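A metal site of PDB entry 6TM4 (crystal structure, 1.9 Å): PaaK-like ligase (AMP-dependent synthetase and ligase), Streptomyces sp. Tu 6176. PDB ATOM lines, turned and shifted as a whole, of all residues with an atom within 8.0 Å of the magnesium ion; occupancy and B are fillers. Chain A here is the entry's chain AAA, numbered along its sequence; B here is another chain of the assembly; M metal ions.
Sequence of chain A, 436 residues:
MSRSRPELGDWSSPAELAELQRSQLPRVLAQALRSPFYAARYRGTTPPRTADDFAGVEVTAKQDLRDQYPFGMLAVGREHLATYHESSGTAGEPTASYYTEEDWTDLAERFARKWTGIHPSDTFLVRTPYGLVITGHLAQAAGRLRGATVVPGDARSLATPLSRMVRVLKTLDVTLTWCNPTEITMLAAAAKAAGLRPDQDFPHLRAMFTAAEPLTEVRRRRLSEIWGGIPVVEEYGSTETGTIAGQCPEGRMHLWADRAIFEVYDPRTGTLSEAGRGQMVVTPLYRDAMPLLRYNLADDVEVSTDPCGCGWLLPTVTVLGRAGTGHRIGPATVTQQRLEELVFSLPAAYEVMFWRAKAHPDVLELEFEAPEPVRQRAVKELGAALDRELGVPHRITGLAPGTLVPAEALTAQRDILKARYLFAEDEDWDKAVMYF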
ATOM      1  N   GLY A  77       2.320 -10.316 -33.986  1.00  0.00           N
ATOM      2  CA  GLY A  77       3.444  -9.767 -34.758  1.00  0.00           C
ATOM      3  C   GLY A  77       4.573  -9.411 -33.802  1.00  0.00           C
ATOM      4  O   GLY A  77       4.300  -8.960 -32.675  1.00  0.00           O
ATOM      5  N   ARG A  78       5.814  -9.580 -34.241  1.00  0.00           N
ATOM      6  CA  ARG A  78       7.005  -9.255 -33.410  1.00  0.00           C
ATOM      7  C   ARG A  78       7.037  -7.768 -33.036  1.00  0.00           C
ATOM      8  O   ARG A  78       7.625  -7.457 -31.986  1.00  0.00           O
ATOM      9  CB  ARG A  78       8.277  -9.759 -34.098  1.00  0.00           C
ATOM     10  CG  ARG A  78       8.376 -11.274 -33.994  1.00  0.00           C
ATOM     11  CD  ARG A  78       9.668 -11.851 -34.504  1.00  0.00           C
ATOM     12  NE  ARG A  78      10.866 -11.248 -33.944  1.00  0.00           N
ATOM     13  CZ  ARG A  78      12.076 -11.687 -34.239  1.00  0.00           C
ATOM     14  NH1 ARG A  78      12.228 -12.676 -35.100  1.00  0.00           N
ATOM     15  NH2 ARG A  78      13.133 -11.113 -33.693  1.00  0.00           N
ATOM     16  N   GLU A  79       6.408  -6.885 -33.823  1.00  0.00           N
ATOM     17  CA  GLU A  79       6.343  -5.420 -33.536  1.00  0.00           C
ATOM     18  C   GLU A  79       5.677  -5.167 -32.160  1.00  0.00           C
ATOM     19  O   GLU A  79       6.023  -4.125 -31.497  1.00  0.00           O
ATOM     20  CB  GLU A  79       5.676  -4.683 -34.723  1.00  0.00           C
ATOM     21  CG  GLU A  79       4.212  -5.018 -34.981  1.00  0.00           C
ATOM     22  CD  GLU A  79       3.885  -6.144 -35.972  1.00  0.00           C
ATOM     23  OE1 GLU A  79       2.749  -6.129 -36.545  1.00  0.00           O
ATOM     24  OE2 GLU A  79       4.723  -7.078 -36.148  1.00  0.00           O
ATOM     25  N   HIS A  80       4.779  -6.065 -31.708  1.00  0.00           N
ATOM     26  CA  HIS A  80       4.018  -5.932 -30.429  1.00  0.00           C
ATOM     27  C   HIS A  80       4.787  -6.507 -29.213  1.00  0.00           C
ATOM     28  O   HIS A  80       4.290  -6.346 -28.087  1.00  0.00           O
ATOM     29  CB  HIS A  80       2.636  -6.599 -30.529  1.00  0.00           C
ATOM     30  CG  HIS A  80       1.816  -6.056 -31.640  1.00  0.00           C
ATOM     31  ND1 HIS A  80       1.414  -4.722 -31.678  1.00  0.00           N
ATOM     32  CD2 HIS A  80       1.321  -6.631 -32.756  1.00  0.00           C
ATOM     33  CE1 HIS A  80       0.704  -4.514 -32.766  1.00  0.00           C
ATOM     34  NE2 HIS A  80       0.629  -5.670 -33.445  1.00  0.00           N
ATOM     35  N   LEU A  81       5.943  -7.168 -29.420  1.00  0.00           N
ATOM     36  CA  LEU A  81       6.767  -7.694 -28.296  1.00  0.00           C
ATOM     37  C   LEU A  81       7.405  -6.526 -27.577  1.00  0.00           C
ATOM     38  O   LEU A  81       7.881  -5.589 -28.254  1.00  0.00           O
ATOM     39  CB  LEU A  81       7.810  -8.689 -28.794  1.00  0.00           C
ATOM     40  CG  LEU A  81       7.242  -9.994 -29.360  1.00  0.00           C
ATOM     41  CD1 LEU A  81       8.380 -10.970 -29.658  1.00  0.00           C
ATOM     42  CD2 LEU A  81       6.227 -10.627 -28.425  1.00  0.00           C
ATOM     43  N   ALA A  82       7.428  -6.575 -26.246  1.00  0.00           N
ATOM     44  CA  ALA A  82       8.167  -5.611 -25.394  1.00  0.00           C
ATOM     45  C   ALA A  82       9.522  -6.211 -25.002  1.00  0.00           C
ATOM     46  O   ALA A  82      10.546  -5.505 -25.128  1.00  0.00           O
ATOM     47  CB  ALA A  82       7.334  -5.280 -24.184  1.00  0.00           C
ATOM     48  N   THR A  83       9.523  -7.431 -24.465  1.00  0.00           N
ATOM     49  CA  THR A  83      10.761  -8.101 -24.000  1.00  0.00           C
ATOM     50  C   THR A  83      10.742  -9.576 -24.400  1.00  0.00           C
ATOM     51  O   THR A  83       9.649 -10.174 -24.667  1.00  0.00           O
ATOM     52  CB  THR A  83      11.007  -7.947 -22.492  1.00  0.00           C
ATOM     53  OG1 THR A  83      10.079  -8.787 -21.799  1.00  0.00           O
ATOM     54  CG2 THR A  83      10.933  -6.521 -21.996  1.00  0.00           C
ATOM     55  N   TYR A  99       6.667 -11.220 -24.170  1.00  0.00           N
ATOM     56  CA  TYR A  99       5.533 -10.495 -23.552  1.00  0.00           C
ATOM     57  C   TYR A  99       5.288  -9.189 -24.305  1.00  0.00           C
ATOM     58  O   TYR A  99       6.299  -8.530 -24.672  1.00  0.00           O
ATOM     59  CB  TYR A  99       5.828 -10.258 -22.073  1.00  0.00           C
ATOM     60  CG  TYR A  99       5.990 -11.541 -21.307  1.00  0.00           C
ATOM     61  CD1 TYR A  99       4.895 -12.298 -20.981  1.00  0.00           C
ATOM     62  CD2 TYR A  99       7.239 -12.036 -20.961  1.00  0.00           C
ATOM     63  CE1 TYR A  99       5.001 -13.499 -20.292  1.00  0.00           C
ATOM     64  CE2 TYR A  99       7.369 -13.236 -20.279  1.00  0.00           C
ATOM     65  CZ  TYR A  99       6.256 -13.970 -19.940  1.00  0.00           C
ATOM     66  OH  TYR A  99       6.323 -15.142 -19.237  1.00  0.00           O
ATOM     67  N   THR A 100       4.023  -8.842 -24.538  1.00  0.00           N
ATOM     68  CA  THR A 100       3.585  -7.482 -24.959  1.00  0.00           C
ATOM     69  C   THR A 100       3.645  -6.571 -23.730  1.00  0.00           C
ATOM     70  O   THR A 100       3.789  -7.117 -22.599  1.00  0.00           O
ATOM     71  CB  THR A 100       2.166  -7.468 -25.529  1.00  0.00           C
ATOM     72  OG1 THR A 100       1.309  -7.798 -24.445  1.00  0.00           O
ATOM     73  CG2 THR A 100       1.959  -8.446 -26.674  1.00  0.00           C
ATOM     74  N   GLU A 101       3.479  -5.261 -23.928  1.00  0.00           N
ATOM     75  CA  GLU A 101       3.390  -4.290 -22.812  1.00  0.00           C
ATOM     76  C   GLU A 101       2.221  -4.686 -21.896  1.00  0.00           C
ATOM     77  O   GLU A 101       2.396  -4.635 -20.672  1.00  0.00           O
ATOM     78  CB  GLU A 101       3.209  -2.857 -23.352  1.00  0.00           C
ATOM     79  CG  GLU A 101       4.459  -2.282 -23.963  1.00  0.00           C
ATOM     80  CD  GLU A 101       5.595  -2.019 -22.974  1.00  0.00           C
ATOM     81  OE1 GLU A 101       6.755  -1.726 -23.436  1.00  0.00           O
ATOM     82  OE2 GLU A 101       5.328  -2.085 -21.743  1.00  0.00           O
ATOM     83  N   HIS B 120      12.884   1.290 -33.607  1.00  0.00           N
ATOM     84  CA  HIS B 120      11.508   1.083 -34.107  1.00  0.00           C
ATOM     85  C   HIS B 120      10.956  -0.216 -33.518  1.00  0.00           C
ATOM     86  O   HIS B 120      11.716  -1.106 -33.117  1.00  0.00           O
ATOM     87  CB  HIS B 120      11.512   1.033 -35.635  1.00  0.00           C
ATOM     88  CG  HIS B 120      12.028   2.281 -36.259  1.00  0.00           C
ATOM     89  ND1 HIS B 120      13.155   2.294 -37.081  1.00  0.00           N
ATOM     90  CD2 HIS B 120      11.634   3.564 -36.130  1.00  0.00           C
ATOM     91  CE1 HIS B 120      13.412   3.533 -37.434  1.00  0.00           C
ATOM     92  NE2 HIS B 120      12.485   4.325 -36.874  1.00  0.00           N
ATOM     93  N   PRO B 121       9.612  -0.366 -33.521  1.00  0.00           N
ATOM     94  CA  PRO B 121       8.975  -1.646 -33.216  1.00  0.00           C
ATOM     95  C   PRO B 121       9.526  -2.837 -34.019  1.00  0.00           C
ATOM     96  O   PRO B 121       9.590  -3.925 -33.469  1.00  0.00           O
ATOM     97  CB  PRO B 121       7.495  -1.344 -33.529  1.00  0.00           C
ATOM     98  CG  PRO B 121       7.364   0.120 -33.206  1.00  0.00           C
ATOM     99  CD  PRO B 121       8.634   0.705 -33.779  1.00  0.00           C
ATOM    100  N   SER B 122       9.968  -2.597 -35.259  1.00  0.00           N
ATOM    101  CA  SER B 122      10.534  -3.630 -36.168  1.00  0.00           C
ATOM    102  C   SER B 122      11.858  -4.164 -35.593  1.00  0.00           C
ATOM    103  O   SER B 122      12.313  -5.196 -36.078  1.00  0.00           O
ATOM    104  CB  SER B 122      10.752  -3.075 -37.573  1.00  0.00           C
ATOM    105  OG  SER B 122      11.585  -1.895 -37.505  1.00  0.00           O
ATOM    106  N   ASP B 123      12.481  -3.463 -34.635  1.00  0.00           N
ATOM    107  CA  ASP B 123      13.806  -3.835 -34.102  1.00  0.00           C
ATOM    108  C   ASP B 123      13.700  -4.873 -32.990  1.00  0.00           C
ATOM    109  O   ASP B 123      12.723  -4.862 -32.194  1.00  0.00           O
ATOM    110  CB  ASP B 123      14.588  -2.619 -33.622  1.00  0.00           C
ATOM    111  CG  ASP B 123      15.114  -1.797 -34.810  1.00  0.00           C
ATOM    112  OD1 ASP B 123      15.745  -2.408 -35.714  1.00  0.00           O
ATOM    113  OD2 ASP B 123      14.877  -0.573 -34.808  1.00  0.00           O
ATOM    114  N   THR B 124      14.704  -5.765 -32.959  1.00  0.00           N
ATOM    115  CA  THR B 124      15.009  -6.669 -31.837  1.00  0.00           C
ATOM    116  C   THR B 124      16.354  -6.209 -31.291  1.00  0.00           C
ATOM    117  O   THR B 124      17.333  -6.245 -32.029  1.00  0.00           O
ATOM    118  CB  THR B 124      14.974  -8.136 -32.299  1.00  0.00           C
ATOM    119  OG1 THR B 124      13.687  -8.428 -32.845  1.00  0.00           O
ATOM    120  CG2 THR B 124      15.277  -9.098 -31.170  1.00  0.00           C
ATOM    121  N   GLY B 144      14.483   1.333 -25.423  1.00  0.00           N
ATOM    122  CA  GLY B 144      13.880   0.288 -26.269  1.00  0.00           C
ATOM    123  C   GLY B 144      12.381   0.191 -26.050  1.00  0.00           C
ATOM    124  O   GLY B 144      11.632   0.044 -27.021  1.00  0.00           O
ATOM    125  N   ARG B 145      11.951   0.228 -24.799  1.00  0.00           N
ATOM    126  CA  ARG B 145      10.519   0.144 -24.452  1.00  0.00           C
ATOM    127  C   ARG B 145       9.847   1.435 -24.925  1.00  0.00           C
ATOM    128  O   ARG B 145       8.759   1.318 -25.487  1.00  0.00           O
ATOM    129  CB  ARG B 145      10.331  -0.032 -22.944  1.00  0.00           C
ATOM    130  CG  ARG B 145      10.767  -1.411 -22.449  1.00  0.00           C
ATOM    131  CD  ARG B 145       9.619  -2.411 -22.357  1.00  0.00           C
ATOM    132  NE  ARG B 145       9.773  -3.089 -21.069  1.00  0.00           N
ATOM    133  CZ  ARG B 145       8.779  -3.476 -20.261  1.00  0.00           C
ATOM    134  NH1 ARG B 145       9.077  -4.052 -19.107  1.00  0.00           N
ATOM    135  NH2 ARG B 145       7.516  -3.299 -20.611  1.00  0.00           N
ATOM    136  N   ARG B 147      10.519   3.262 -27.483  1.00  0.00           N
ATOM    137  CA  ARG B 147      10.395   3.291 -28.952  1.00  0.00           C
ATOM    138  C   ARG B 147       9.738   2.002 -29.474  1.00  0.00           C
ATOM    139  O   ARG B 147       9.556   1.910 -30.704  1.00  0.00           O
ATOM    140  CB  ARG B 147      11.765   3.497 -29.589  1.00  0.00           C
ATOM    141  CG  ARG B 147      12.340   4.881 -29.395  1.00  0.00           C
ATOM    142  CD  ARG B 147      11.671   5.939 -30.261  1.00  0.00           C
ATOM    143  NE  ARG B 147      12.135   7.246 -29.780  1.00  0.00           N
ATOM    144  CZ  ARG B 147      11.416   8.144 -29.070  1.00  0.00           C
ATOM    145  NH1 ARG B 147      10.148   7.946 -28.749  1.00  0.00           N
ATOM    146  NH2 ARG B 147      11.969   9.275 -28.703  1.00  0.00           N
ATOM    147  N   GLY B 148       9.380   1.050 -28.605  1.00  0.00           N
ATOM    148  CA  GLY B 148       8.596  -0.151 -28.972  1.00  0.00           C
ATOM    149  C   GLY B 148       9.458  -1.290 -29.504  1.00  0.00           C
ATOM    150  O   GLY B 148       8.899  -2.225 -30.079  1.00  0.00           O
ATOM    151  N   ALA B 149      10.781  -1.230 -29.369  1.00  0.00           N
ATOM    152  CA  ALA B 149      11.653  -2.312 -29.880  1.00  0.00           C
ATOM    153  C   ALA B 149      11.540  -3.491 -28.903  1.00  0.00           C
ATOM    154  O   ALA B 149      11.305  -3.244 -27.719  1.00  0.00           O
ATOM    155  CB  ALA B 149      13.073  -1.829 -30.028  1.00  0.00           C
ATOM    156  N   THR B 150      11.655  -4.726 -29.386  1.00  0.00           N
ATOM    157  CA  THR B 150      11.784  -5.919 -28.533  1.00  0.00           C
ATOM    158  C   THR B 150      13.141  -5.885 -27.837  1.00  0.00           C
ATOM    159  O   THR B 150      14.154  -5.893 -28.534  1.00  0.00           O
ATOM    160  CB  THR B 150      11.690  -7.223 -29.329  1.00  0.00           C
ATOM    161  OG1 THR B 150      10.402  -7.224 -29.972  1.00  0.00           O
ATOM    162  CG2 THR B 150      11.828  -8.433 -28.449  1.00  0.00           C
ATOM    163  N   VAL B 151      13.139  -5.766 -26.524  1.00  0.00           N
ATOM    164  CA  VAL B 151      14.383  -5.764 -25.711  1.00  0.00           C
ATOM    165  C   VAL B 151      14.735  -7.204 -25.331  1.00  0.00           C
ATOM    166  O   VAL B 151      13.883  -7.869 -24.755  1.00  0.00           O
ATOM    167  CB  VAL B 151      14.232  -4.882 -24.473  1.00  0.00           C
ATOM    168  CG1 VAL B 151      15.447  -4.974 -23.585  1.00  0.00           C
ATOM    169  CG2 VAL B 151      13.941  -3.458 -24.903  1.00  0.00           C
HETATM  170 MG    MG M   1       7.642  -4.003 -29.851  1.00  0.00          MG
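O of Leu 81 lies close to OG1 of Thr 150 of chain B (3.5 Å).
Residues that only touch the magnesium ion: His 80 (3.9 Å).
Along chain A the residues within 4 Å of the magnesium ion span positions 79 to 81.
The magnesium ion is bound by O of Gly 148 of chain B (2.2 Å), O of Leu 81 (2.3 Å) and O of Glu 79 (2.3 Å).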
